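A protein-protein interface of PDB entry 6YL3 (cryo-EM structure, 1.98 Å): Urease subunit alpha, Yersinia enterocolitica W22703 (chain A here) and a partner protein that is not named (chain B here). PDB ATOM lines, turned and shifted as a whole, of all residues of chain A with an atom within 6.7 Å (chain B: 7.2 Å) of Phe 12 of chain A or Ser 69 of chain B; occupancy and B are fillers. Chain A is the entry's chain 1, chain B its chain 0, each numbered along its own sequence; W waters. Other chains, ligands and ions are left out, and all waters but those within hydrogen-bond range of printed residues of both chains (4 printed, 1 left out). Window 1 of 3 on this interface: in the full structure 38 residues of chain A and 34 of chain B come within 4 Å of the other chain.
NE2 of His 43 of chain B is in hydrogen-bond range of OE1 of Glu 40 of chain A (3.1 Å).
NH2 of Arg 64 of chain B is in salt-bridge range of OE1 of Glu 40 of chain A (3.3 Å).
O of Glu 41 of chain A lies within hydrogen-bond range of OG of Ser 69 of chain B.
O of Ser 42 of chain B sits close to NH1 of Arg 64 of chain B (3.5 Å).
OG of Ser 42 of chain B is in hydrogen-bond range of N of Thr 70 of chain B (3.2 Å).
The backbone carbonyl oxygen of Phe 12 of chain A is in hydrogen-bond range of the side-chain amino group of Lys 85 of chain A (2.7 Å).
N of Gly 39 of chain A is in hydrogen-bond range of OE2 of Glu 41 of chain A.
The backbone carbonyl oxygen of Glu 41 of chain A is in hydrogen-bond range of the side-chain hydroxyl of Ser 49 of chain A, at 2.8 Å.
N of Val 43 of chain A lies within hydrogen-bond range of OG of Ser 49 of chain A (2.9 Å).
Among the printed residues, merely in contact across the chains: Ile 3 of chain A with Phe 19 of chain B, Ile 3 of chain A with Ser 68 of chain B, Leu 11 of chain A with Ser 68 of chain B, Leu 11 of chain A with Thr 70 of chain B, Leu 11 of chain A with Thr 71 of chain B, Phe 12 of chain A with Ser 69 of chain B, Phe 12 of chain A with Thr 70 of chain B, Gly 39 of chain A with Phe 19 of chain B, Gly 39 of chain A with Asn 20 of chain B, Gly 39 of chain A with Arg 64 of chain B, Gly 39 of chain A with Ser 69 of chain B, Val 43 of chain A with Thr 70 of chain B, Lys 48 of chain A with Thr 70 of chain B, Ser 49 of chain A with His 43 of chain B and Ser 49 of chain A with Ser 69 of chain B.
Of chain B, only Ser 69 and Thr 70 come within 4 Å of Phe 12 of chain A.
Arg 36 of chain A touches none of the printed residues of chain B.
Of the printed residues of chain B, Glu 41 of chain A touches Ser 69.
Thr 72 of chain A touches none of the printed residues of chain B.
Of the printed residues of chain A, Arg 64 of chain B touches Gly 39 and Glu 40.
Of chain A, only Phe 12 (3.3 Å), Gly 39 (3.7 Å), Glu 41 (2.5 Å) and Ser 49 (3.9 Å) come within 4 Å of Ser 69 of chain B.
The nearest printed residue of chain A that does not touch Ser 68 of chain B is Phe 12 of chain A (5.1 Å).
Of the 25 printed residues of chain A, 9 touch a printed residue of chain B.
Printed residues of chain A that touch a printed residue of chain B: Ile 3, Leu 11, Phe 12, Gly 39, Glu 40, Glu 41, Val 43, Lys 48 and Ser 49.
Hydrophobic or aromatic side chains of chain A within 4 Å of the printed part of chain B: Ile 3, Leu 11, Phe 12 and Val 43.
Printed residues of chain B that touch a printed residue of chain A: Phe 19, Asn 20, His 43, Arg 64, Ser 68, Ser 69, Thr 70 and Thr 71.
Along chain B the printed residues that touch a printed residue of chain A span positions 19 to 71.
Among the printed residues, Asp or Glu carboxylates within 4 Å of a Lys or Arg side-chain nitrogen of the other chain: Glu 40 of chain A with Arg 64 of chain B (3.3 Å).
Water W2 lies within hydrogen-bond range of OE2 of Glu 40 of chain A (2.9 Å) and NE of Arg 64 of chain B (2.9 Å).
Water W1 lies within hydrogen-bond range of N of His 43 of chain B (3.0 Å), N of Ser 42 of chain B (3.1 Å) and O of Lys 48 of chain A (3.4 Å).
Water W3 lies within hydrogen-bond range of OE1 of Glu 41 of chain A (3.0 Å) and N of Ser 69 of chain B (3.0 Å).
Water W4 bridges the side-chain hydroxyl of Thr 70 of chain B and the backbone carbonyl oxygen of Leu 11 of chain A.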
ATOM      1  N   ILE A   3       0.251  13.037  32.572  1.00  0.00           N
ATOM      2  CA  ILE A   3      -0.428  12.207  31.548  1.00  0.00           C
ATOM      3  C   ILE A   3       0.656  11.381  30.839  1.00  0.00           C
ATOM      4  O   ILE A   3       1.688  11.869  30.607  1.00  0.00           O
ATOM      5  CB  ILE A   3      -1.278  13.048  30.548  1.00  0.00           C
ATOM      6  CG1 ILE A   3      -2.061  12.243  29.498  1.00  0.00           C
ATOM      7  CG2 ILE A   3      -0.455  14.102  29.836  1.00  0.00           C
ATOM      8  CD1 ILE A   3      -2.586  13.084  28.373  1.00  0.00           C
ATOM      9  N   GLU A   7      -1.332   8.508  25.853  1.00  0.00           N
ATOM     10  CA  GLU A   7      -2.605   9.161  26.016  1.00  0.00           C
ATOM     11  C   GLU A   7      -2.577  10.564  25.429  1.00  0.00           C
ATOM     12  O   GLU A   7      -3.489  10.937  24.724  1.00  0.00           O
ATOM     13  CB  GLU A   7      -2.982   9.181  27.455  1.00  0.00           C
ATOM     14  CG  GLU A   7      -4.223   9.728  27.738  1.00  0.00           C
ATOM     15  CD  GLU A   7      -5.386   8.908  27.153  1.00  0.00           C
ATOM     16  OE1 GLU A   7      -5.158   7.761  26.721  1.00  0.00           O
ATOM     17  OE2 GLU A   7      -6.499   9.448  27.093  1.00  0.00           O
ATOM     18  N   TYR A   8      -1.504  11.243  25.682  1.00  0.00           N
ATOM     19  CA  TYR A   8      -1.199  12.546  25.106  1.00  0.00           C
ATOM     20  C   TYR A   8      -1.283  12.453  23.569  1.00  0.00           C
ATOM     21  O   TYR A   8      -1.977  13.246  23.017  1.00  0.00           O
ATOM     22  CB  TYR A   8       0.174  12.998  25.565  1.00  0.00           C
ATOM     23  CG  TYR A   8       0.364  14.422  25.179  1.00  0.00           C
ATOM     24  CD1 TYR A   8      -0.183  15.430  25.944  1.00  0.00           C
ATOM     25  CD2 TYR A   8       0.945  14.733  23.963  1.00  0.00           C
ATOM     26  CE1 TYR A   8      -0.004  16.748  25.612  1.00  0.00           C
ATOM     27  CE2 TYR A   8       1.109  16.042  23.589  1.00  0.00           C
ATOM     28  CZ  TYR A   8       0.530  17.017  24.370  1.00  0.00           C
ATOM     29  OH  TYR A   8       0.638  18.279  24.029  1.00  0.00           O
ATOM     30  N   ALA A   9      -0.612  11.473  22.937  1.00  0.00           N
ATOM     31  CA  ALA A   9      -0.472  11.306  21.512  1.00  0.00           C
ATOM     32  C   ALA A   9      -1.813  11.118  20.848  1.00  0.00           C
ATOM     33  O   ALA A   9      -2.133  11.781  19.877  1.00  0.00           O
ATOM     34  CB  ALA A   9       0.516  10.187  21.174  1.00  0.00           C
ATOM     35  N   GLY A  10      -2.606  10.262  21.427  1.00  0.00           N
ATOM     36  CA  GLY A  10      -3.951  10.073  21.097  1.00  0.00           C
ATOM     37  C   GLY A  10      -4.826  11.286  21.105  1.00  0.00           C
ATOM     38  O   GLY A  10      -5.747  11.370  20.335  1.00  0.00           O
ATOM     39  N   LEU A  11      -4.539  12.218  21.919  1.00  0.00           N
ATOM     40  CA  LEU A  11      -5.257  13.473  21.938  1.00  0.00           C
ATOM     41  C   LEU A  11      -4.695  14.539  20.986  1.00  0.00           C
ATOM     42  O   LEU A  11      -5.429  15.358  20.454  1.00  0.00           O
ATOM     43  CB  LEU A  11      -5.356  14.047  23.356  1.00  0.00           C
ATOM     44  CG  LEU A  11      -6.392  13.610  24.400  1.00  0.00           C
ATOM     45  CD1 LEU A  11      -6.015  14.322  25.771  1.00  0.00           C
ATOM     46  CD2 LEU A  11      -7.749  13.824  24.139  1.00  0.00           C
ATOM     47  N   PHE A  12      -3.448  14.602  20.881  1.00  0.00           N
ATOM     48  CA  PHE A  12      -2.717  15.712  20.341  1.00  0.00           C
ATOM     49  C   PHE A  12      -1.641  15.386  19.314  1.00  0.00           C
ATOM     50  O   PHE A  12      -0.978  16.271  18.815  1.00  0.00           O
ATOM     51  CB  PHE A  12      -2.138  16.485  21.451  1.00  0.00           C
ATOM     52  CG  PHE A  12      -3.077  16.839  22.537  1.00  0.00           C
ATOM     53  CD1 PHE A  12      -4.134  17.620  22.361  1.00  0.00           C
ATOM     54  CD2 PHE A  12      -2.823  16.516  23.762  1.00  0.00           C
ATOM     55  CE1 PHE A  12      -4.868  17.931  23.305  1.00  0.00           C
ATOM     56  CE2 PHE A  12      -3.600  16.958  24.746  1.00  0.00           C
ATOM     57  CZ  PHE A  12      -4.578  17.608  24.447  1.00  0.00           C
ATOM     58  N   GLY A  13      -1.485  14.181  19.001  1.00  0.00           N
ATOM     59  CA  GLY A  13      -0.404  13.647  18.316  1.00  0.00           C
ATOM     60  C   GLY A  13       0.966  13.638  18.923  1.00  0.00           C
ATOM     61  O   GLY A  13       1.151  13.934  20.073  1.00  0.00           O
ATOM     62  N   PRO A  14       1.959  13.279  18.126  1.00  0.00           N
ATOM     63  CA  PRO A  14       3.322  13.154  18.640  1.00  0.00           C
ATOM     64  C   PRO A  14       4.016  14.390  19.098  1.00  0.00           C
ATOM     65  O   PRO A  14       3.804  15.472  18.595  1.00  0.00           O
ATOM     66  CB  PRO A  14       4.015  12.496  17.484  1.00  0.00           C
ATOM     67  CG  PRO A  14       3.235  12.671  16.398  1.00  0.00           C
ATOM     68  CD  PRO A  14       1.930  12.742  16.752  1.00  0.00           C
ATOM     69  N   THR A  15       4.831  14.329  20.147  1.00  0.00           N
ATOM     70  CA  THR A  15       5.605  15.496  20.609  1.00  0.00           C
ATOM     71  C   THR A  15       7.124  15.256  20.496  1.00  0.00           C
ATOM     72  O   THR A  15       7.462  14.231  20.138  1.00  0.00           O
ATOM     73  CB  THR A  15       5.072  15.900  21.998  1.00  0.00           C
ATOM     74  OG1 THR A  15       5.748  17.082  22.369  1.00  0.00           O
ATOM     75  CG2 THR A  15       5.314  14.854  23.058  1.00  0.00           C
ATOM     76  N   ARG A  36       4.390  24.288  20.810  1.00  0.00           N
ATOM     77  CA  ARG A  36       3.040  24.693  21.251  1.00  0.00           C
ATOM     78  C   ARG A  36       2.739  24.287  22.684  1.00  0.00           C
ATOM     79  O   ARG A  36       1.670  23.722  22.834  1.00  0.00           O
ATOM     80  CB  ARG A  36       1.906  24.325  20.279  1.00  0.00           C
ATOM     81  CG  ARG A  36       2.057  23.170  19.332  1.00  0.00           C
ATOM     82  CD  ARG A  36       1.304  21.957  19.720  1.00  0.00           C
ATOM     83  NE  ARG A  36       2.040  21.129  20.571  1.00  0.00           N
ATOM     84  CZ  ARG A  36       1.541  20.188  21.326  1.00  0.00           C
ATOM     85  NH1 ARG A  36       0.259  19.914  21.269  1.00  0.00           N
ATOM     86  NH2 ARG A  36       2.291  19.507  22.157  1.00  0.00           N
ATOM     87  N   GLY A  39      -0.698  21.581  28.104  1.00  0.00           N
ATOM     88  CA  GLY A  39      -1.862  22.041  28.863  1.00  0.00           C
ATOM     89  C   GLY A  39      -2.757  23.094  28.232  1.00  0.00           C
ATOM     90  O   GLY A  39      -3.825  23.057  28.588  1.00  0.00           O
ATOM     91  N   GLU A  40      -2.438  23.795  27.150  1.00  0.00           N
ATOM     92  CA  GLU A  40      -3.367  24.807  26.552  1.00  0.00           C
ATOM     93  C   GLU A  40      -3.621  24.527  25.054  1.00  0.00           C
ATOM     94  O   GLU A  40      -3.840  25.403  24.339  1.00  0.00           O
ATOM     95  CB  GLU A  40      -2.794  26.207  26.711  1.00  0.00           C
ATOM     96  CG  GLU A  40      -2.495  26.626  28.139  1.00  0.00           C
ATOM     97  CD  GLU A  40      -3.704  27.083  28.941  1.00  0.00           C
ATOM     98  OE1 GLU A  40      -4.795  26.670  28.614  1.00  0.00           O
ATOM     99  OE2 GLU A  40      -3.541  27.948  29.836  1.00  0.00           O
ATOM    100  N   GLU A  41      -3.690  23.299  24.687  1.00  0.00           N
ATOM    101  CA  GLU A  41      -3.681  22.735  23.361  1.00  0.00           C
ATOM    102  C   GLU A  41      -4.976  23.095  22.603  1.00  0.00           C
ATOM    103  O   GLU A  41      -6.057  22.888  23.096  1.00  0.00           O
ATOM    104  CB  GLU A  41      -3.422  21.254  23.377  1.00  0.00           C
ATOM    105  CG  GLU A  41      -2.084  20.612  23.686  1.00  0.00           C
ATOM    106  CD  GLU A  41      -1.829  20.577  25.168  1.00  0.00           C
ATOM    107  OE1 GLU A  41      -2.707  21.020  25.889  1.00  0.00           O
ATOM    108  OE2 GLU A  41      -0.771  20.185  25.554  1.00  0.00           O
ATOM    109  N   SER A  42      -4.845  23.806  21.533  1.00  0.00           N
ATOM    110  CA  SER A  42      -5.893  24.267  20.634  1.00  0.00           C
ATOM    111  C   SER A  42      -6.405  23.224  19.685  1.00  0.00           C
ATOM    112  O   SER A  42      -5.746  22.871  18.757  1.00  0.00           O
ATOM    113  CB  SER A  42      -5.398  25.524  19.945  1.00  0.00           C
ATOM    114  OG  SER A  42      -4.393  25.383  19.192  1.00  0.00           O
ATOM    115  N   VAL A  43      -7.633  22.788  19.896  1.00  0.00           N
ATOM    116  CA  VAL A  43      -8.383  21.843  19.101  1.00  0.00           C
ATOM    117  C   VAL A  43      -9.834  22.292  18.890  1.00  0.00           C
ATOM    118  O   VAL A  43     -10.509  22.822  19.781  1.00  0.00           O
ATOM    119  CB  VAL A  43      -8.275  20.378  19.588  1.00  0.00           C
ATOM    120  CG1 VAL A  43      -8.790  19.214  18.611  1.00  0.00           C
ATOM    121  CG2 VAL A  43      -6.933  20.060  20.035  1.00  0.00           C
ATOM    122  N   LYS A  48     -14.489  21.387  23.192  1.00  0.00           N
ATOM    123  CA  LYS A  48     -13.104  21.552  23.096  1.00  0.00           C
ATOM    124  C   LYS A  48     -12.676  22.991  23.284  1.00  0.00           C
ATOM    125  O   LYS A  48     -13.417  23.833  23.735  1.00  0.00           O
ATOM    126  CB  LYS A  48     -12.643  20.879  21.856  1.00  0.00           C
ATOM    127  CG  LYS A  48     -12.857  19.454  21.642  1.00  0.00           C
ATOM    128  CD  LYS A  48     -11.844  18.907  20.792  1.00  0.00           C
ATOM    129  CE  LYS A  48     -12.266  17.631  20.237  1.00  0.00           C
ATOM    130  NZ  LYS A  48     -12.629  16.780  21.050  1.00  0.00           N
ATOM    131  N   SER A  49     -11.451  23.263  22.985  1.00  0.00           N
ATOM    132  CA  SER A  49     -10.736  24.456  23.418  1.00  0.00           C
ATOM    133  C   SER A  49     -10.935  25.703  22.549  1.00  0.00           C
ATOM    134  O   SER A  49     -10.948  26.786  23.078  1.00  0.00           O
ATOM    135  CB  SER A  49      -9.254  24.218  23.583  1.00  0.00           C
ATOM    136  OG  SER A  49      -8.619  23.764  22.478  1.00  0.00           O
ATOM    137  N   THR A  72      -3.656  23.166  13.395  1.00  0.00           N
ATOM    138  CA  THR A  72      -3.367  22.821  14.769  1.00  0.00           C
ATOM    139  C   THR A  72      -2.678  21.512  14.986  1.00  0.00           C
ATOM    140  O   THR A  72      -3.041  20.487  14.496  1.00  0.00           O
ATOM    141  CB  THR A  72      -4.631  22.823  15.675  1.00  0.00           C
ATOM    142  OG1 THR A  72      -5.523  21.767  15.368  1.00  0.00           O
ATOM    143  CG2 THR A  72      -5.191  23.843  15.750  1.00  0.00           C
ATOM    144  N   ASN A  73      -1.749  21.562  15.850  1.00  0.00           N
ATOM    145  CA  ASN A  73      -1.048  20.458  16.359  1.00  0.00           C
ATOM    146  C   ASN A  73      -0.402  19.566  15.260  1.00  0.00           C
ATOM    147  O   ASN A  73      -0.450  18.370  15.293  1.00  0.00           O
ATOM    148  CB  ASN A  73      -1.868  19.685  17.363  1.00  0.00           C
ATOM    149  CG  ASN A  73      -2.391  20.538  18.447  1.00  0.00           C
ATOM    150  OD1 ASN A  73      -1.720  21.169  19.164  1.00  0.00           O
ATOM    151  ND2 ASN A  73      -3.593  20.599  18.452  1.00  0.00           N
ATOM    152  N   VAL A  74       0.262  20.191  14.360  1.00  0.00           N
ATOM    153  CA  VAL A  74       0.787  19.604  13.135  1.00  0.00           C
ATOM    154  C   VAL A  74       2.267  19.496  13.156  1.00  0.00           C
ATOM    155  O   VAL A  74       2.994  20.374  13.563  1.00  0.00           O
ATOM    156  CB  VAL A  74       0.329  20.287  11.819  1.00  0.00           C
ATOM    157  CG1 VAL A  74       0.906  21.530  11.524  1.00  0.00           C
ATOM    158  CG2 VAL A  74       0.152  19.386  10.771  1.00  0.00           C
ATOM    159  N   LYS A  85       6.742  20.324  15.603  1.00  0.00           N
ATOM    160  CA  LYS A  85       5.362  20.325  16.046  1.00  0.00           C
ATOM    161  C   LYS A  85       4.961  21.703  16.491  1.00  0.00           C
ATOM    162  O   LYS A  85       5.576  22.291  17.339  1.00  0.00           O
ATOM    163  CB  LYS A  85       5.061  19.253  17.007  1.00  0.00           C
ATOM    164  CG  LYS A  85       3.706  18.924  17.405  1.00  0.00           C
ATOM    165  CD  LYS A  85       2.926  18.011  16.625  1.00  0.00           C
ATOM    166  CE  LYS A  85       1.743  17.595  17.573  1.00  0.00           C
ATOM    167  NZ  LYS A  85       1.356  16.564  17.422  1.00  0.00           N
ATOM    168  N   GLY A 125      -4.629  19.189  12.574  1.00  0.00           N
ATOM    169  CA  GLY A 125      -3.344  18.636  12.213  1.00  0.00           C
ATOM    170  C   GLY A 125      -2.698  17.585  13.073  1.00  0.00           C
ATOM    171  O   GLY A 125      -1.640  17.067  12.741  1.00  0.00           O
ATOM    172  N   GLU A 126      -3.448  17.138  14.062  1.00  0.00           N
ATOM    173  CA  GLU A 126      -2.968  16.300  15.154  1.00  0.00           C
ATOM    174  C   GLU A 126      -2.259  15.069  14.665  1.00  0.00           C
ATOM    175  O   GLU A 126      -1.186  14.744  15.122  1.00  0.00           O
ATOM    176  CB  GLU A 126      -4.138  15.942  16.109  1.00  0.00           C
ATOM    177  CG  GLU A 126      -4.657  17.159  16.964  1.00  0.00           C
ATOM    178  CD  GLU A 126      -5.213  18.417  16.346  1.00  0.00           C
ATOM    179  OE1 GLU A 126      -4.880  19.479  16.767  1.00  0.00           O
ATOM    180  OE2 GLU A 126      -6.032  18.422  15.490  1.00  0.00           O
ATOM    181  N   HIS A 127      -2.870  14.359  13.797  1.00  0.00           N
ATOM    182  CA  HIS A 127      -2.344  13.144  13.234  1.00  0.00           C
ATOM    183  C   HIS A 127      -1.771  13.361  11.794  1.00  0.00           C
ATOM    184  O   HIS A 127      -1.628  12.419  11.069  1.00  0.00           O
ATOM    185  CB  HIS A 127      -3.396  12.050  13.368  1.00  0.00           C
ATOM    186  CG  HIS A 127      -3.880  11.885  14.774  1.00  0.00           C
ATOM    187  ND1 HIS A 127      -3.019  11.545  15.790  1.00  0.00           N
ATOM    188  CD2 HIS A 127      -5.074  12.118  15.347  1.00  0.00           C
ATOM    189  CE1 HIS A 127      -3.680  11.546  16.924  1.00  0.00           C
ATOM    190  NE2 HIS A 127      -4.934  11.861  16.673  1.00  0.00           N
ATOM    191  N   PHE B  19       1.693  18.694  32.702  1.00  0.00           N
ATOM    192  CA  PHE B  19       0.979  19.898  32.397  1.00  0.00           C
ATOM    193  C   PHE B  19       0.335  20.547  33.628  1.00  0.00           C
ATOM    194  O   PHE B  19       0.023  19.902  34.588  1.00  0.00           O
ATOM    195  CB  PHE B  19      -0.139  19.709  31.281  1.00  0.00           C
ATOM    196  CG  PHE B  19      -1.215  18.813  31.605  1.00  0.00           C
ATOM    197  CD1 PHE B  19      -1.022  17.513  31.657  1.00  0.00           C
ATOM    198  CD2 PHE B  19      -2.468  19.227  31.848  1.00  0.00           C
ATOM    199  CE1 PHE B  19      -1.939  16.748  31.976  1.00  0.00           C
ATOM    200  CE2 PHE B  19      -3.356  18.370  32.136  1.00  0.00           C
ATOM    201  CZ  PHE B  19      -3.076  17.157  32.215  1.00  0.00           C
ATOM    202  N   ASN B  20       0.171  21.840  33.522  1.00  0.00           N
ATOM    203  CA  ASN B  20      -0.459  22.781  34.414  1.00  0.00           C
ATOM    204  C   ASN B  20       0.260  22.875  35.787  1.00  0.00           C
ATOM    205  O   ASN B  20      -0.254  23.460  36.685  1.00  0.00           O
ATOM    206  CB  ASN B  20      -1.940  22.473  34.508  1.00  0.00           C
ATOM    207  CG  ASN B  20      -2.733  22.724  33.284  1.00  0.00           C
ATOM    208  OD1 ASN B  20      -2.410  23.448  32.422  1.00  0.00           O
ATOM    209  ND2 ASN B  20      -3.849  22.117  33.261  1.00  0.00           N
ATOM    210  N   SER B  42     -12.768  21.633  29.546  1.00  0.00           N
ATOM    211  CA  SER B  42     -11.539  22.001  30.190  1.00  0.00           C
ATOM    212  C   SER B  42     -11.335  23.496  30.358  1.00  0.00           C
ATOM    213  O   SER B  42     -10.675  23.900  31.286  1.00  0.00           O
ATOM    214  CB  SER B  42     -10.341  21.368  29.432  1.00  0.00           C
ATOM    215  OG  SER B  42     -10.262  21.656  28.119  1.00  0.00           O
ATOM    216  N   HIS B  43     -11.745  24.249  29.334  1.00  0.00           N
ATOM    217  CA  HIS B  43     -11.594  25.727  29.199  1.00  0.00           C
ATOM    218  C   HIS B  43     -12.829  26.527  29.506  1.00  0.00           C
ATOM    219  O   HIS B  43     -12.742  27.670  29.399  1.00  0.00           O
ATOM    220  CB  HIS B  43     -10.968  26.256  27.913  1.00  0.00           C
ATOM    221  CG  HIS B  43      -9.576  25.884  27.924  1.00  0.00           C
ATOM    222  ND1 HIS B  43      -9.211  24.753  27.394  1.00  0.00           N
ATOM    223  CD2 HIS B  43      -8.495  26.363  28.535  1.00  0.00           C
ATOM    224  CE1 HIS B  43      -8.011  24.463  27.699  1.00  0.00           C
ATOM    225  NE2 HIS B  43      -7.573  25.408  28.373  1.00  0.00           N
ATOM    226  N   ARG B  64     -11.178  27.290  35.795  1.00  0.00           N
ATOM    227  CA  ARG B  64     -11.297  26.178  34.927  1.00  0.00           C
ATOM    228  C   ARG B  64     -10.865  24.877  35.575  1.00  0.00           C
ATOM    229  O   ARG B  64     -10.076  24.814  36.475  1.00  0.00           O
ATOM    230  CB  ARG B  64     -10.568  26.385  33.641  1.00  0.00           C
ATOM    231  CG  ARG B  64      -9.192  26.069  33.392  1.00  0.00           C
ATOM    232  CD  ARG B  64      -8.642  26.464  32.079  1.00  0.00           C
ATOM    233  NE  ARG B  64      -7.263  26.127  31.797  1.00  0.00           N
ATOM    234  CZ  ARG B  64      -6.681  24.999  31.625  1.00  0.00           C
ATOM    235  NH1 ARG B  64      -7.258  24.008  31.774  1.00  0.00           N
ATOM    236  NH2 ARG B  64      -5.437  24.970  31.320  1.00  0.00           N
ATOM    237  N   LEU B  65     -11.336  23.861  35.004  1.00  0.00           N
ATOM    238  CA  LEU B  65     -10.993  22.522  35.328  1.00  0.00           C
ATOM    239  C   LEU B  65      -9.569  22.137  34.918  1.00  0.00           C
ATOM    240  O   LEU B  65      -9.178  22.327  33.777  1.00  0.00           O
ATOM    241  CB  LEU B  65     -11.920  21.587  34.733  1.00  0.00           C
ATOM    242  CG  LEU B  65     -13.406  21.285  35.062  1.00  0.00           C
ATOM    243  CD1 LEU B  65     -14.209  20.628  34.069  1.00  0.00           C
ATOM    244  CD2 LEU B  65     -13.454  20.713  36.334  1.00  0.00           C
ATOM    245  N   ASN B  66      -8.861  21.527  35.845  1.00  0.00           N
ATOM    246  CA  ASN B  66      -7.494  21.102  35.798  1.00  0.00           C
ATOM    247  C   ASN B  66      -7.404  19.702  35.237  1.00  0.00           C
ATOM    248  O   ASN B  66      -7.075  18.776  35.864  1.00  0.00           O
ATOM    249  CB  ASN B  66      -6.827  21.167  37.150  1.00  0.00           C
ATOM    250  CG  ASN B  66      -5.343  21.152  37.043  1.00  0.00           C
ATOM    251  OD1 ASN B  66      -4.813  21.595  36.114  1.00  0.00           O
ATOM    252  ND2 ASN B  66      -4.706  20.667  37.991  1.00  0.00           N
ATOM    253  N   ILE B  67      -7.843  19.617  34.020  1.00  0.00           N
ATOM    254  CA  ILE B  67      -7.852  18.448  33.188  1.00  0.00           C
ATOM    255  C   ILE B  67      -7.174  18.749  31.843  1.00  0.00           C
ATOM    256  O   ILE B  67      -6.898  19.888  31.505  1.00  0.00           O
ATOM    257  CB  ILE B  67      -9.278  17.881  33.016  1.00  0.00           C
ATOM    258  CG1 ILE B  67     -10.147  18.823  32.230  1.00  0.00           C
ATOM    259  CG2 ILE B  67      -9.868  17.492  34.306  1.00  0.00           C
ATOM    260  CD1 ILE B  67     -11.417  18.466  31.994  1.00  0.00           C
ATOM    261  N   SER B  68      -6.965  17.693  31.072  1.00  0.00           N
ATOM    262  CA  SER B  68      -6.404  17.775  29.741  1.00  0.00           C
ATOM    263  C   SER B  68      -7.246  18.649  28.836  1.00  0.00           C
ATOM    264  O   SER B  68      -8.441  18.546  28.827  1.00  0.00           O
ATOM    265  CB  SER B  68      -6.265  16.428  29.077  1.00  0.00           C
ATOM    266  OG  SER B  68      -5.283  15.718  29.529  1.00  0.00           O
ATOM    267  N   SER B  69      -6.601  19.612  28.241  1.00  0.00           N
ATOM    268  CA  SER B  69      -7.139  20.319  27.104  1.00  0.00           C
ATOM    269  C   SER B  69      -7.870  19.347  26.199  1.00  0.00           C
ATOM    270  O   SER B  69      -7.441  18.240  25.935  1.00  0.00           O
ATOM    271  CB  SER B  69      -6.133  21.186  26.343  1.00  0.00           C
ATOM    272  OG  SER B  69      -6.730  21.658  25.202  1.00  0.00           O
ATOM    273  N   THR B  70      -9.032  19.750  25.932  1.00  0.00           N
ATOM    274  CA  THR B  70     -10.035  19.235  25.060  1.00  0.00           C
ATOM    275  C   THR B  70     -10.944  18.215  25.712  1.00  0.00           C
ATOM    276  O   THR B  70     -11.938  17.855  25.147  1.00  0.00           O
ATOM    277  CB  THR B  70      -9.421  18.699  23.762  1.00  0.00           C
ATOM    278  OG1 THR B  70      -8.635  17.573  23.930  1.00  0.00           O
ATOM    279  CG2 THR B  70      -8.720  19.788  23.085  1.00  0.00           C
ATOM    280  N   THR B  71     -10.649  17.789  26.893  1.00  0.00           N
ATOM    281  CA  THR B  71     -11.433  16.794  27.568  1.00  0.00           C
ATOM    282  C   THR B  71     -12.472  17.518  28.474  1.00  0.00           C
ATOM    283  O   THR B  71     -12.426  18.712  28.663  1.00  0.00           O
ATOM    284  CB  THR B  71     -10.567  15.809  28.325  1.00  0.00           C
ATOM    285  OG1 THR B  71     -10.082  16.387  29.515  1.00  0.00           O
ATOM    286  CG2 THR B  71      -9.420  15.186  27.463  1.00  0.00           C
ATOM    287  N   ALA B  72     -13.303  16.736  29.075  1.00  0.00           N
ATOM    288  CA  ALA B  72     -14.479  17.126  29.812  1.00  0.00           C
ATOM    289  C   ALA B  72     -14.774  16.219  31.017  1.00  0.00           C
ATOM    290  O   ALA B  72     -14.382  15.075  31.077  1.00  0.00           O
ATOM    291  CB  ALA B  72     -15.734  17.143  28.948  1.00  0.00           C
HETATM  292  O   HOH W   1     -13.417  23.330  27.082  1.00  0.00           O
HETATM  293  O   HOH W   2      -6.327  28.427  30.339  1.00  0.00           O
HETATM  294  O   HOH W   3      -3.725  18.895  27.701  1.00  0.00           O
HETATM  295  O   HOH W   4      -8.242  16.285  21.219  1.00  0.00           O
